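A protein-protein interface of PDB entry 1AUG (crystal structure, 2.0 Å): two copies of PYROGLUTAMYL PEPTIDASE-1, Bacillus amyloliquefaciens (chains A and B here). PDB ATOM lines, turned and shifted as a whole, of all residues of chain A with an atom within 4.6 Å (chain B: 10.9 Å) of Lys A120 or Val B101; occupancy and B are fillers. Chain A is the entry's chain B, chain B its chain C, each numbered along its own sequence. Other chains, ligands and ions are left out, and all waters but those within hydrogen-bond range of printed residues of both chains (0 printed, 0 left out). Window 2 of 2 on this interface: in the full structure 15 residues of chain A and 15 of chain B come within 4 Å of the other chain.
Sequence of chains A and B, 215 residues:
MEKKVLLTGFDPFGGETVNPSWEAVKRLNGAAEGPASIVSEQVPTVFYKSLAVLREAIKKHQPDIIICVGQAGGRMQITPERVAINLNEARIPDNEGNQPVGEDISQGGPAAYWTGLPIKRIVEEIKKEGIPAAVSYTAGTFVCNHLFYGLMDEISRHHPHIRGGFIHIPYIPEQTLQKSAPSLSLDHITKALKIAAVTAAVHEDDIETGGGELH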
ATOM      1  N   ARG A  82      -7.766   4.014 -18.309  1.00  0.00           N
ATOM      2  CA  ARG A  82      -6.818   4.110 -17.216  1.00  0.00           C
ATOM      3  C   ARG A  82      -5.707   3.083 -17.356  1.00  0.00           C
ATOM      4  O   ARG A  82      -4.615   3.408 -16.899  1.00  0.00           O
ATOM      5  CB  ARG A  82      -7.507   3.880 -15.867  1.00  0.00           C
ATOM      6  CG  ARG A  82      -6.739   4.242 -14.545  1.00  0.00           C
ATOM      7  CD  ARG A  82      -7.025   5.698 -14.239  1.00  0.00           C
ATOM      8  NE  ARG A  82      -6.820   6.215 -12.900  1.00  0.00           N
ATOM      9  CZ  ARG A  82      -7.828   6.500 -12.027  1.00  0.00           C
ATOM     10  NH1 ARG A  82      -9.132   6.359 -12.296  1.00  0.00           N
ATOM     11  NH2 ARG A  82      -7.531   6.975 -10.804  1.00  0.00           N
ATOM     12  N   PRO A 118      -4.092  13.298 -17.760  1.00  0.00           N
ATOM     13  CA  PRO A 118      -4.923  13.646 -16.645  1.00  0.00           C
ATOM     14  C   PRO A 118      -6.386  13.251 -16.997  1.00  0.00           C
ATOM     15  O   PRO A 118      -7.257  14.111 -17.152  1.00  0.00           O
ATOM     16  CB  PRO A 118      -4.545  15.100 -16.512  1.00  0.00           C
ATOM     17  CG  PRO A 118      -4.438  15.601 -17.905  1.00  0.00           C
ATOM     18  CD  PRO A 118      -3.686  14.472 -18.509  1.00  0.00           C
ATOM     19  N   ILE A 119      -6.752  11.950 -17.013  1.00  0.00           N
ATOM     20  CA  ILE A 119      -8.048  11.516 -17.499  1.00  0.00           C
ATOM     21  C   ILE A 119      -9.269  11.901 -16.694  1.00  0.00           C
ATOM     22  O   ILE A 119     -10.337  12.052 -17.267  1.00  0.00           O
ATOM     23  CB  ILE A 119      -8.076   9.996 -17.720  1.00  0.00           C
ATOM     24  CG1 ILE A 119      -7.859   9.183 -16.460  1.00  0.00           C
ATOM     25  CG2 ILE A 119      -6.990   9.672 -18.725  1.00  0.00           C
ATOM     26  CD1 ILE A 119      -8.283   7.753 -16.852  1.00  0.00           C
ATOM     27  N   LYS A 120      -9.203  12.127 -15.389  1.00  0.00           N
ATOM     28  CA  LYS A 120     -10.368  12.589 -14.666  1.00  0.00           C
ATOM     29  C   LYS A 120     -10.690  14.019 -15.019  1.00  0.00           C
ATOM     30  O   LYS A 120     -11.835  14.436 -15.120  1.00  0.00           O
ATOM     31  CB  LYS A 120     -10.143  12.523 -13.199  1.00  0.00           C
ATOM     32  CG  LYS A 120     -10.136  11.089 -12.732  1.00  0.00           C
ATOM     33  CD  LYS A 120      -9.900  11.176 -11.255  1.00  0.00           C
ATOM     34  CE  LYS A 120     -10.113   9.810 -10.651  1.00  0.00           C
ATOM     35  NZ  LYS A 120     -10.161   9.910  -9.197  1.00  0.00           N
ATOM     36  N   ARG A 121      -9.647  14.783 -15.269  1.00  0.00           N
ATOM     37  CA  ARG A 121      -9.766  16.167 -15.625  1.00  0.00           C
ATOM     38  C   ARG A 121     -10.367  16.228 -17.012  1.00  0.00           C
ATOM     39  O   ARG A 121     -11.311  16.985 -17.227  1.00  0.00           O
ATOM     40  CB  ARG A 121      -8.372  16.743 -15.558  1.00  0.00           C
ATOM     41  CG  ARG A 121      -8.391  18.210 -15.360  1.00  0.00           C
ATOM     42  CD  ARG A 121      -7.019  18.658 -14.973  1.00  0.00           C
ATOM     43  NE  ARG A 121      -7.254  19.941 -14.331  1.00  0.00           N
ATOM     44  CZ  ARG A 121      -6.710  20.294 -13.165  1.00  0.00           C
ATOM     45  NH1 ARG A 121      -5.876  19.495 -12.501  1.00  0.00           N
ATOM     46  NH2 ARG A 121      -7.109  21.421 -12.582  1.00  0.00           N
ATOM     47  N   ILE A 122      -9.863  15.418 -17.949  1.00  0.00           N
ATOM     48  CA  ILE A 122     -10.390  15.337 -19.283  1.00  0.00           C
ATOM     49  C   ILE A 122     -11.894  14.988 -19.262  1.00  0.00           C
ATOM     50  O   ILE A 122     -12.698  15.635 -19.951  1.00  0.00           O
ATOM     51  CB  ILE A 122      -9.571  14.298 -20.039  1.00  0.00           C
ATOM     52  CG1 ILE A 122      -8.172  14.882 -20.299  1.00  0.00           C
ATOM     53  CG2 ILE A 122     -10.266  13.900 -21.346  1.00  0.00           C
ATOM     54  CD1 ILE A 122      -7.240  13.902 -21.029  1.00  0.00           C
ATOM     55  N   VAL A 123     -12.291  14.001 -18.434  1.00  0.00           N
ATOM     56  CA  VAL A 123     -13.666  13.573 -18.333  1.00  0.00           C
ATOM     57  C   VAL A 123     -14.522  14.735 -17.855  1.00  0.00           C
ATOM     58  O   VAL A 123     -15.494  15.057 -18.512  1.00  0.00           O
ATOM     59  CB  VAL A 123     -13.684  12.353 -17.391  1.00  0.00           C
ATOM     60  CG1 VAL A 123     -15.063  11.983 -16.957  1.00  0.00           C
ATOM     61  CG2 VAL A 123     -13.197  11.143 -18.190  1.00  0.00           C
ATOM     62  N   GLU A 124     -14.176  15.451 -16.815  1.00  0.00           N
ATOM     63  CA  GLU A 124     -14.960  16.574 -16.352  1.00  0.00           C
ATOM     64  C   GLU A 124     -15.080  17.731 -17.344  1.00  0.00           C
ATOM     65  O   GLU A 124     -16.145  18.349 -17.464  1.00  0.00           O
ATOM     66  CB  GLU A 124     -14.377  17.097 -15.046  1.00  0.00           C
ATOM     67  CG  GLU A 124     -14.469  16.072 -13.937  1.00  0.00           C
ATOM     68  CD  GLU A 124     -15.889  15.580 -13.664  1.00  0.00           C
ATOM     69  OE1 GLU A 124     -16.737  16.392 -13.282  1.00  0.00           O
ATOM     70  OE2 GLU A 124     -16.143  14.382 -13.824  1.00  0.00           O
ATOM     71  N   ASP A 206      -3.540  15.514 -12.413  1.00  0.00           N
ATOM     72  CA  ASP A 206      -4.956  15.222 -12.568  1.00  0.00           C
ATOM     73  C   ASP A 206      -5.764  15.681 -11.340  1.00  0.00           C
ATOM     74  O   ASP A 206      -5.246  16.070 -10.300  1.00  0.00           O
ATOM     75  CB  ASP A 206      -5.112  13.702 -12.807  1.00  0.00           C
ATOM     76  CG  ASP A 206      -6.444  13.215 -13.410  1.00  0.00           C
ATOM     77  OD1 ASP A 206      -7.283  14.068 -13.685  1.00  0.00           O
ATOM     78  OD2 ASP A 206      -6.633  12.000 -13.618  1.00  0.00           O
ATOM     79  N   ILE A 207      -7.076  15.722 -11.516  1.00  0.00           N
ATOM     80  CA  ILE A 207      -8.078  15.953 -10.491  1.00  0.00           C
ATOM     81  C   ILE A 207      -8.267  14.604  -9.743  1.00  0.00           C
ATOM     82  O   ILE A 207      -7.853  13.563 -10.271  1.00  0.00           O
ATOM     83  CB  ILE A 207      -9.282  16.515 -11.369  1.00  0.00           C
ATOM     84  CG1 ILE A 207      -9.594  17.881 -10.874  1.00  0.00           C
ATOM     85  CG2 ILE A 207     -10.575  15.749 -11.286  1.00  0.00           C
ATOM     86  CD1 ILE A 207      -8.409  18.852 -10.818  1.00  0.00           C
ATOM     87  N   GLU A 208      -8.830  14.512  -8.527  1.00  0.00           N
ATOM     88  CA  GLU A 208      -9.133  13.235  -7.871  1.00  0.00           C
ATOM     89  C   GLU A 208     -10.648  13.162  -7.639  1.00  0.00           C
ATOM     90  O   GLU A 208     -11.121  13.727  -6.647  1.00  0.00           O
ATOM     91  N   THR A 209     -11.425  12.456  -8.482  1.00  0.00           N
ATOM     92  CA  THR A 209     -12.899  12.383  -8.444  1.00  0.00           C
ATOM     93  C   THR A 209     -13.380  10.990  -8.948  1.00  0.00           C
ATOM     94  O   THR A 209     -12.892  10.615 -10.021  1.00  0.00           O
ATOM     95  CB  THR A 209     -13.509  13.525  -9.383  1.00  0.00           C
ATOM     96  OG1 THR A 209     -12.899  14.791  -9.089  1.00  0.00           O
ATOM     97  CG2 THR A 209     -15.025  13.638  -9.193  1.00  0.00           C
ATOM     98  N   GLY A 210     -14.246  10.134  -8.372  1.00  0.00           N
ATOM     99  CA  GLY A 210     -14.675   8.908  -9.062  1.00  0.00           C
ATOM    100  C   GLY A 210     -15.439   7.941  -8.169  1.00  0.00           C
ATOM    101  O   GLY A 210     -15.880   8.381  -7.099  1.00  0.00           O
ATOM    102  N   PHE B  47     -12.712  -2.502   2.806  1.00  0.00           N
ATOM    103  CA  PHE B  47     -11.352  -2.270   2.368  1.00  0.00           C
ATOM    104  C   PHE B  47     -10.432  -2.522   3.548  1.00  0.00           C
ATOM    105  O   PHE B  47     -10.775  -2.207   4.685  1.00  0.00           O
ATOM    106  CB  PHE B  47     -11.103  -0.805   1.912  1.00  0.00           C
ATOM    107  CG  PHE B  47     -11.680  -0.487   0.556  1.00  0.00           C
ATOM    108  CD1 PHE B  47     -11.013  -0.892  -0.584  1.00  0.00           C
ATOM    109  CD2 PHE B  47     -12.923   0.128   0.479  1.00  0.00           C
ATOM    110  CE1 PHE B  47     -11.607  -0.698  -1.813  1.00  0.00           C
ATOM    111  CE2 PHE B  47     -13.520   0.320  -0.771  1.00  0.00           C
ATOM    112  CZ  PHE B  47     -12.856  -0.095  -1.914  1.00  0.00           C
ATOM    113  N   TYR B  48      -9.260  -3.083   3.253  1.00  0.00           N
ATOM    114  CA  TYR B  48      -8.124  -3.288   4.196  1.00  0.00           C
ATOM    115  C   TYR B  48      -8.433  -4.428   5.157  1.00  0.00           C
ATOM    116  O   TYR B  48      -7.688  -5.400   5.140  1.00  0.00           O
ATOM    117  CB  TYR B  48      -7.761  -2.020   5.077  1.00  0.00           C
ATOM    118  CG  TYR B  48      -7.918  -0.665   4.358  1.00  0.00           C
ATOM    119  CD1 TYR B  48      -7.281  -0.407   3.130  1.00  0.00           C
ATOM    120  CD2 TYR B  48      -8.813   0.285   4.903  1.00  0.00           C
ATOM    121  CE1 TYR B  48      -7.560   0.786   2.456  1.00  0.00           C
ATOM    122  CE2 TYR B  48      -9.099   1.479   4.225  1.00  0.00           C
ATOM    123  CZ  TYR B  48      -8.475   1.722   2.993  1.00  0.00           C
ATOM    124  OH  TYR B  48      -8.783   2.881   2.289  1.00  0.00           O
ATOM    125  N   ASN B  86      -3.933  -2.222  -9.223  1.00  0.00           N
ATOM    126  CA  ASN B  86      -3.497  -1.656  -7.958  1.00  0.00           C
ATOM    127  C   ASN B  86      -4.200  -0.351  -7.632  1.00  0.00           C
ATOM    128  O   ASN B  86      -3.568   0.682  -7.479  1.00  0.00           O
ATOM    129  CB  ASN B  86      -1.971  -1.481  -8.048  1.00  0.00           C
ATOM    130  CG  ASN B  86      -1.288  -1.075  -6.760  1.00  0.00           C
ATOM    131  OD1 ASN B  86      -1.816  -1.174  -5.665  1.00  0.00           O
ATOM    132  ND2 ASN B  86      -0.101  -0.561  -6.795  1.00  0.00           N
ATOM    133  N   LEU B  87      -5.500  -0.328  -7.416  1.00  0.00           N
ATOM    134  CA  LEU B  87      -6.188   0.938  -7.241  1.00  0.00           C
ATOM    135  C   LEU B  87      -7.425   0.678  -6.431  1.00  0.00           C
ATOM    136  O   LEU B  87      -8.130  -0.272  -6.745  1.00  0.00           O
ATOM    137  CB  LEU B  87      -6.584   1.459  -8.617  1.00  0.00           C
ATOM    138  CG  LEU B  87      -6.805   2.951  -9.019  1.00  0.00           C
ATOM    139  CD1 LEU B  87      -7.986   2.942  -9.939  1.00  0.00           C
ATOM    140  CD2 LEU B  87      -7.066   3.885  -7.881  1.00  0.00           C
ATOM    141  N   ASN B  88      -7.672   1.512  -5.428  1.00  0.00           N
ATOM    142  CA  ASN B  88      -8.910   1.526  -4.676  1.00  0.00           C
ATOM    143  C   ASN B  88      -9.655   2.781  -5.144  1.00  0.00           C
ATOM    144  O   ASN B  88      -9.149   3.898  -4.941  1.00  0.00           O
ATOM    145  CB  ASN B  88      -8.646   1.666  -3.188  1.00  0.00           C
ATOM    146  CG  ASN B  88      -7.970   0.498  -2.526  1.00  0.00           C
ATOM    147  OD1 ASN B  88      -8.159  -0.647  -2.880  1.00  0.00           O
ATOM    148  ND2 ASN B  88      -7.094   0.723  -1.582  1.00  0.00           N
ATOM    149  N   GLU B  89     -10.811   2.705  -5.785  1.00  0.00           N
ATOM    150  CA  GLU B  89     -11.521   3.873  -6.296  1.00  0.00           C
ATOM    151  C   GLU B  89     -13.000   3.560  -6.046  1.00  0.00           C
ATOM    152  O   GLU B  89     -13.678   2.849  -6.796  1.00  0.00           O
ATOM    153  CB  GLU B  89     -11.207   3.969  -7.738  1.00  0.00           C
ATOM    154  CG  GLU B  89     -11.855   5.103  -8.487  1.00  0.00           C
ATOM    155  CD  GLU B  89     -11.129   6.438  -8.473  1.00  0.00           C
ATOM    156  OE1 GLU B  89      -9.923   6.541  -8.736  1.00  0.00           O
ATOM    157  OE2 GLU B  89     -11.825   7.409  -8.250  1.00  0.00           O
ATOM    158  N   ALA B  90     -13.455   3.980  -4.877  1.00  0.00           N
ATOM    159  CA  ALA B  90     -14.770   3.643  -4.422  1.00  0.00           C
ATOM    160  C   ALA B  90     -15.806   4.694  -4.807  1.00  0.00           C
ATOM    161  O   ALA B  90     -15.764   5.809  -4.268  1.00  0.00           O
ATOM    162  CB  ALA B  90     -14.744   3.497  -2.904  1.00  0.00           C
ATOM    163  N   ARG B  91     -16.766   4.247  -5.635  1.00  0.00           N
ATOM    164  CA  ARG B  91     -17.931   5.052  -5.975  1.00  0.00           C
ATOM    165  C   ARG B  91     -18.881   5.159  -4.795  1.00  0.00           C
ATOM    166  O   ARG B  91     -19.532   6.175  -4.575  1.00  0.00           O
ATOM    167  CB  ARG B  91     -18.717   4.473  -7.188  1.00  0.00           C
ATOM    168  CG  ARG B  91     -18.450   3.033  -7.737  1.00  0.00           C
ATOM    169  CD  ARG B  91     -19.074   1.797  -6.998  1.00  0.00           C
ATOM    170  NE  ARG B  91     -18.701   0.503  -7.598  1.00  0.00           N
ATOM    171  CZ  ARG B  91     -19.274  -0.687  -7.286  1.00  0.00           C
ATOM    172  NH1 ARG B  91     -20.277  -0.817  -6.405  1.00  0.00           N
ATOM    173  NH2 ARG B  91     -18.842  -1.799  -7.896  1.00  0.00           N
ATOM    174  N   ILE B  92     -18.985   4.121  -3.972  1.00  0.00           N
ATOM    175  CA  ILE B  92     -19.891   4.069  -2.843  1.00  0.00           C
ATOM    176  C   ILE B  92     -19.036   3.670  -1.629  1.00  0.00           C
ATOM    177  O   ILE B  92     -17.951   3.123  -1.855  1.00  0.00           O
ATOM    178  CB  ILE B  92     -20.978   3.073  -3.382  1.00  0.00           C
ATOM    179  CG1 ILE B  92     -22.276   3.542  -2.824  1.00  0.00           C
ATOM    180  CG2 ILE B  92     -20.742   1.612  -3.038  1.00  0.00           C
ATOM    181  CD1 ILE B  92     -22.685   4.895  -3.481  1.00  0.00           C
ATOM    182  N   PRO B  93     -19.353   3.968  -0.376  1.00  0.00           N
ATOM    183  CA  PRO B  93     -18.539   3.571   0.763  1.00  0.00           C
ATOM    184  C   PRO B  93     -18.711   2.092   1.038  1.00  0.00           C
ATOM    185  O   PRO B  93     -19.779   1.538   0.715  1.00  0.00           O
ATOM    186  CB  PRO B  93     -19.012   4.453   1.896  1.00  0.00           C
ATOM    187  CG  PRO B  93     -20.437   4.775   1.517  1.00  0.00           C
ATOM    188  CD  PRO B  93     -20.371   4.929   0.000  1.00  0.00           C
ATOM    189  N   ASP B  94     -17.707   1.444   1.623  1.00  0.00           N
ATOM    190  CA  ASP B  94     -17.849   0.052   1.991  1.00  0.00           C
ATOM    191  C   ASP B  94     -18.723  -0.107   3.221  1.00  0.00           C
ATOM    192  O   ASP B  94     -19.196   0.883   3.774  1.00  0.00           O
ATOM    193  CB  ASP B  94     -16.447  -0.533   2.231  1.00  0.00           C
ATOM    194  CG  ASP B  94     -15.571  -0.115   3.426  1.00  0.00           C
ATOM    195  OD1 ASP B  94     -16.069   0.393   4.421  1.00  0.00           O
ATOM    196  OD2 ASP B  94     -14.367  -0.339   3.374  1.00  0.00           O
ATOM    197  N   GLY B  97     -17.969   2.457   6.006  1.00  0.00           N
ATOM    198  CA  GLY B  97     -17.866   3.865   5.656  1.00  0.00           C
ATOM    199  C   GLY B  97     -16.591   4.282   4.956  1.00  0.00           C
ATOM    200  O   GLY B  97     -16.447   5.452   4.650  1.00  0.00           O
ATOM    201  N   ASN B  98     -15.629   3.417   4.641  1.00  0.00           N
ATOM    202  CA  ASN B  98     -14.419   3.836   3.922  1.00  0.00           C
ATOM    203  C   ASN B  98     -14.768   4.053   2.454  1.00  0.00           C
ATOM    204  O   ASN B  98     -15.418   3.213   1.818  1.00  0.00           O
ATOM    205  CB  ASN B  98     -13.304   2.772   3.969  1.00  0.00           C
ATOM    206  CG  ASN B  98     -12.937   2.324   5.352  1.00  0.00           C
ATOM    207  OD1 ASN B  98     -12.515   3.124   6.163  1.00  0.00           O
ATOM    208  ND2 ASN B  98     -13.045   1.066   5.738  1.00  0.00           N
ATOM    209  N   GLN B  99     -14.347   5.171   1.873  1.00  0.00           N
ATOM    210  CA  GLN B  99     -14.559   5.420   0.463  1.00  0.00           C
ATOM    211  C   GLN B  99     -13.227   5.955  -0.087  1.00  0.00           C
ATOM    212  O   GLN B  99     -13.062   7.151  -0.312  1.00  0.00           O
ATOM    213  CB  GLN B  99     -15.686   6.431   0.310  1.00  0.00           C
ATOM    214  CG  GLN B  99     -16.175   6.474  -1.109  1.00  0.00           C
ATOM    215  CD  GLN B  99     -17.417   7.312  -1.343  1.00  0.00           C
ATOM    216  OE1 GLN B  99     -18.099   7.812  -0.444  1.00  0.00           O
ATOM    217  NE2 GLN B  99     -17.748   7.455  -2.614  1.00  0.00           N
ATOM    218  N   PRO B 100     -12.176   5.153  -0.291  1.00  0.00           N
ATOM    219  CA  PRO B 100     -10.936   5.575  -0.937  1.00  0.00           C
ATOM    220  C   PRO B 100     -11.086   5.999  -2.391  1.00  0.00           C
ATOM    221  O   PRO B 100     -11.784   5.383  -3.193  1.00  0.00           O
ATOM    222  CB  PRO B 100     -10.021   4.385  -0.754  1.00  0.00           C
ATOM    223  CG  PRO B 100     -10.983   3.229  -0.810  1.00  0.00           C
ATOM    224  CD  PRO B 100     -12.112   3.737   0.049  1.00  0.00           C
ATOM    225  N   VAL B 101     -10.391   7.034  -2.791  1.00  0.00           N
ATOM    226  CA  VAL B 101     -10.468   7.527  -4.155  1.00  0.00           C
ATOM    227  C   VAL B 101      -9.020   7.660  -4.595  1.00  0.00           C
ATOM    228  O   VAL B 101      -8.204   8.260  -3.901  1.00  0.00           O
ATOM    229  CB  VAL B 101     -11.195   8.900  -4.179  1.00  0.00           C
ATOM    230  CG1 VAL B 101     -11.274   9.389  -5.608  1.00  0.00           C
ATOM    231  CG2 VAL B 101     -12.644   8.793  -3.722  1.00  0.00           C
ATOM    232  N   GLY B 102      -8.652   7.083  -5.728  1.00  0.00           N
ATOM    233  CA  GLY B 102      -7.305   7.214  -6.242  1.00  0.00           C
ATOM    234  C   GLY B 102      -6.196   6.664  -5.336  1.00  0.00           C
ATOM    235  O   GLY B 102      -5.058   7.138  -5.399  1.00  0.00           O
ATOM    236  N   GLU B 103      -6.452   5.615  -4.552  1.00  0.00           N
ATOM    237  CA  GLU B 103      -5.465   5.133  -3.615  1.00  0.00           C
ATOM    238  C   GLU B 103      -4.815   3.850  -4.078  1.00  0.00           C
ATOM    239  O   GLU B 103      -5.481   2.966  -4.596  1.00  0.00           O
ATOM    240  CB  GLU B 103      -6.189   4.967  -2.332  1.00  0.00           C
ATOM    241  CG  GLU B 103      -5.404   4.359  -1.206  1.00  0.00           C
ATOM    242  CD  GLU B 103      -6.273   4.053   0.005  1.00  0.00           C
ATOM    243  OE1 GLU B 103      -6.867   2.981   0.036  1.00  0.00           O
ATOM    244  OE2 GLU B 103      -6.357   4.881   0.921  1.00  0.00           O
ATOM    245  N   ASP B 104      -3.509   3.718  -3.948  1.00  0.00           N
ATOM    246  CA  ASP B 104      -2.796   2.500  -4.288  1.00  0.00           C
ATOM    247  C   ASP B 104      -3.160   1.419  -3.310  1.00  0.00           C
ATOM    248  O   ASP B 104      -3.441   1.744  -2.158  1.00  0.00           O
ATOM    249  CB  ASP B 104      -1.325   2.684  -4.189  1.00  0.00           C
ATOM    250  CG  ASP B 104      -0.635   3.368  -5.364  1.00  0.00           C
ATOM    251  OD1 ASP B 104      -1.160   3.426  -6.484  1.00  0.00           O
ATOM    252  OD2 ASP B 104       0.484   3.827  -5.150  1.00  0.00           O
ATOM    253  N   ILE B 105      -3.241   0.142  -3.703  1.00  0.00           N
ATOM    254  CA  ILE B 105      -3.497  -0.897  -2.713  1.00  0.00           C
ATOM    255  C   ILE B 105      -2.103  -1.163  -2.128  1.00  0.00           C
ATOM    256  O   ILE B 105      -1.913  -1.162  -0.912  1.00  0.00           O
ATOM    257  CB  ILE B 105      -4.122  -2.173  -3.420  1.00  0.00           C
ATOM    258  CG1 ILE B 105      -5.533  -1.917  -3.887  1.00  0.00           C
ATOM    259  CG2 ILE B 105      -4.208  -3.323  -2.421  1.00  0.00           C
ATOM    260  CD1 ILE B 105      -6.044  -2.865  -4.949  1.00  0.00           C
ATOM    261  N   GLN B 107       1.635   0.406  -2.146  1.00  0.00           N
ATOM    262  CA  GLN B 107       2.466   1.543  -2.559  1.00  0.00           C
ATOM    263  C   GLN B 107       3.744   0.952  -3.167  1.00  0.00           C
ATOM    264  O   GLN B 107       4.476   0.202  -2.507  1.00  0.00           O
ATOM    265  CB  GLN B 107       2.765   2.423  -1.323  1.00  0.00           C
ATOM    266  CG  GLN B 107       1.638   3.302  -0.677  1.00  0.00           C
ATOM    267  CD  GLN B 107       0.301   2.637  -0.256  1.00  0.00           C
ATOM    268  OE1 GLN B 107      -0.774   3.226  -0.447  1.00  0.00           O
ATOM    269  NE2 GLN B 107       0.237   1.448   0.366  1.00  0.00           N
ATOM    270  N   THR B 141     -13.018  -1.500  -9.223  1.00  0.00           N
ATOM    271  CA  THR B 141     -12.026  -0.829  -8.424  1.00  0.00           C
ATOM    272  C   THR B 141     -12.551  -0.741  -7.000  1.00  0.00           C
ATOM    273  O   THR B 141     -12.058   0.045  -6.198  1.00  0.00           O
ATOM    274  CB  THR B 141     -11.765   0.576  -9.002  1.00  0.00           C
ATOM    275  OG1 THR B 141     -13.025   1.204  -9.087  1.00  0.00           O
ATOM    276  CG2 THR B 141     -11.150   0.581 -10.366  1.00  0.00           C
ATOM    277  N   PHE B 142     -13.556  -1.564  -6.649  1.00  0.00           N
ATOM    278  CA  PHE B 142     -14.166  -1.585  -5.333  1.00  0.00           C
ATOM    279  C   PHE B 142     -13.525  -2.711  -4.513  1.00  0.00           C
ATOM    280  O   PHE B 142     -12.407  -3.140  -4.856  1.00  0.00           O
ATOM    281  CB  PHE B 142     -15.662  -1.776  -5.566  1.00  0.00           C
ATOM    282  CG  PHE B 142     -16.511  -1.465  -4.349  1.00  0.00           C
ATOM    283  CD1 PHE B 142     -16.383  -0.244  -3.692  1.00  0.00           C
ATOM    284  CD2 PHE B 142     -17.362  -2.450  -3.860  1.00  0.00           C
ATOM    285  CE1 PHE B 142     -17.103  -0.001  -2.521  1.00  0.00           C
ATOM    286  CE2 PHE B 142     -18.074  -2.204  -2.685  1.00  0.00           C
ATOM    287  CZ  PHE B 142     -17.947  -0.986  -2.016  1.00  0.00           C
ATOM    288  N   HIS B 146      -9.934  -5.175  -4.889  1.00  0.00           N
ATOM    289  CA  HIS B 146      -9.043  -4.975  -3.787  1.00  0.00           C
ATOM    290  C   HIS B 146      -8.619  -6.310  -3.257  1.00  0.00           C
ATOM    291  O   HIS B 146      -7.425  -6.524  -3.071  1.00  0.00           O
ATOM    292  CB  HIS B 146      -9.789  -4.194  -2.765  1.00  0.00           C
ATOM    293  CG  HIS B 146      -9.073  -3.863  -1.491  1.00  0.00           C
ATOM    294  ND1 HIS B 146      -8.135  -2.976  -1.415  1.00  0.00           N
ATOM    295  CD2 HIS B 146      -9.295  -4.370  -0.257  1.00  0.00           C
ATOM    296  CE1 HIS B 146      -7.751  -2.902  -0.177  1.00  0.00           C
ATOM    297  NE2 HIS B 146      -8.453  -3.750   0.524  1.00  0.00           N
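Of the 13 printed residues of chain A, 4 touch a printed residue of chain B. Of the 24 printed residues of chain B, 3 touch a printed residue of chain A. Among the printed residues, 6 pairs touch across the chains. Among the printed residues, Asp or Glu carboxylates within 4 Å of a Lys or Arg side-chain nitrogen of the other chain: Arg A82 with Glu B89 and Lys A120 with Glu B89.
Among the printed residues, pairs that only touch across the chains: Gly A210 with Glu B89, Lys A120 with Val B101, Thr A209 with Glu B89 and Gly A210 with Ala B90.
Of the printed residues of chain B, Arg A82 touches Glu B89. Pro A118 touches none of the printed residues of chain B. Of chain B, only Glu B89 and Val B101 come within 4 Å of Lys A120. Arg A121 touches none of the printed residues of chain B. No residue of chain B comes within 4 Å of Ile A122. Val A123 touches none of the printed residues of chain B. No residue of chain B comes within 4 Å of Glu A124. No residue of chain B comes within 4 Å of Ile A207. No residue of chain B comes within 4 Å of Glu A208. Of chain B, only Glu B89 comes within 4 Å of Thr A209. Gly A210 touches just these residues of chain B: Glu B89 and Ala B90. Of the printed residues of chain A, Glu B89 touches Arg A82 (3.2 Å), Lys A120 (3.1 Å), Thr A209 (3.8 Å) and Gly A210 (3.3 Å). Of the printed residues of chain A, Ala B90 touches Gly A210 (3.8 Å). Val B101 touches just one residue of chain A: Lys A120 (3.8 Å). Asp B104 touches none of the printed residues of chain A. The nearest printed residue of chain B that does not touch Arg A82 is Leu B87 (4.1 Å).
NH2 of Arg A82 is in salt-bridge range of OE1 of Glu B89 (3.2 Å). The side-chain amino group (NZ) of Lys A120 is in salt-bridge range of the side-chain carboxylate (OE2) of Glu B89, 3.1 Å away.
The backbone NH (N) of Lys A120 is in hydrogen-bond range of the side-chain carboxylate (OD2) of Asp A206 (3.1 Å). NZ of Lys A120 lies within hydrogen-bond range of O of Thr A209, 2.9 Å away. The side-chain carboxylate (OE1) of Glu B89 sits at hydrogen-bond distance from the backbone NH (N) of Gly B102 (3.3 Å). The backbone carbonyl oxygen of Glu B89 sits at hydrogen-bond distance from the side-chain hydroxyl of Thr B141, at 2.9 Å. The backbone carbonyl oxygen of Ala B90 sits at hydrogen-bond distance from the side-chain amide nitrogen of Gln B99, at 3.1 Å. N of Ala B90 is in hydrogen-bond range of O of Pro B100, 2.8 Å away.
No position is printed for both chains. Of the 6 pairs that touch across the chains among the printed residues, none has its exchanged pair printed and touching as well.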
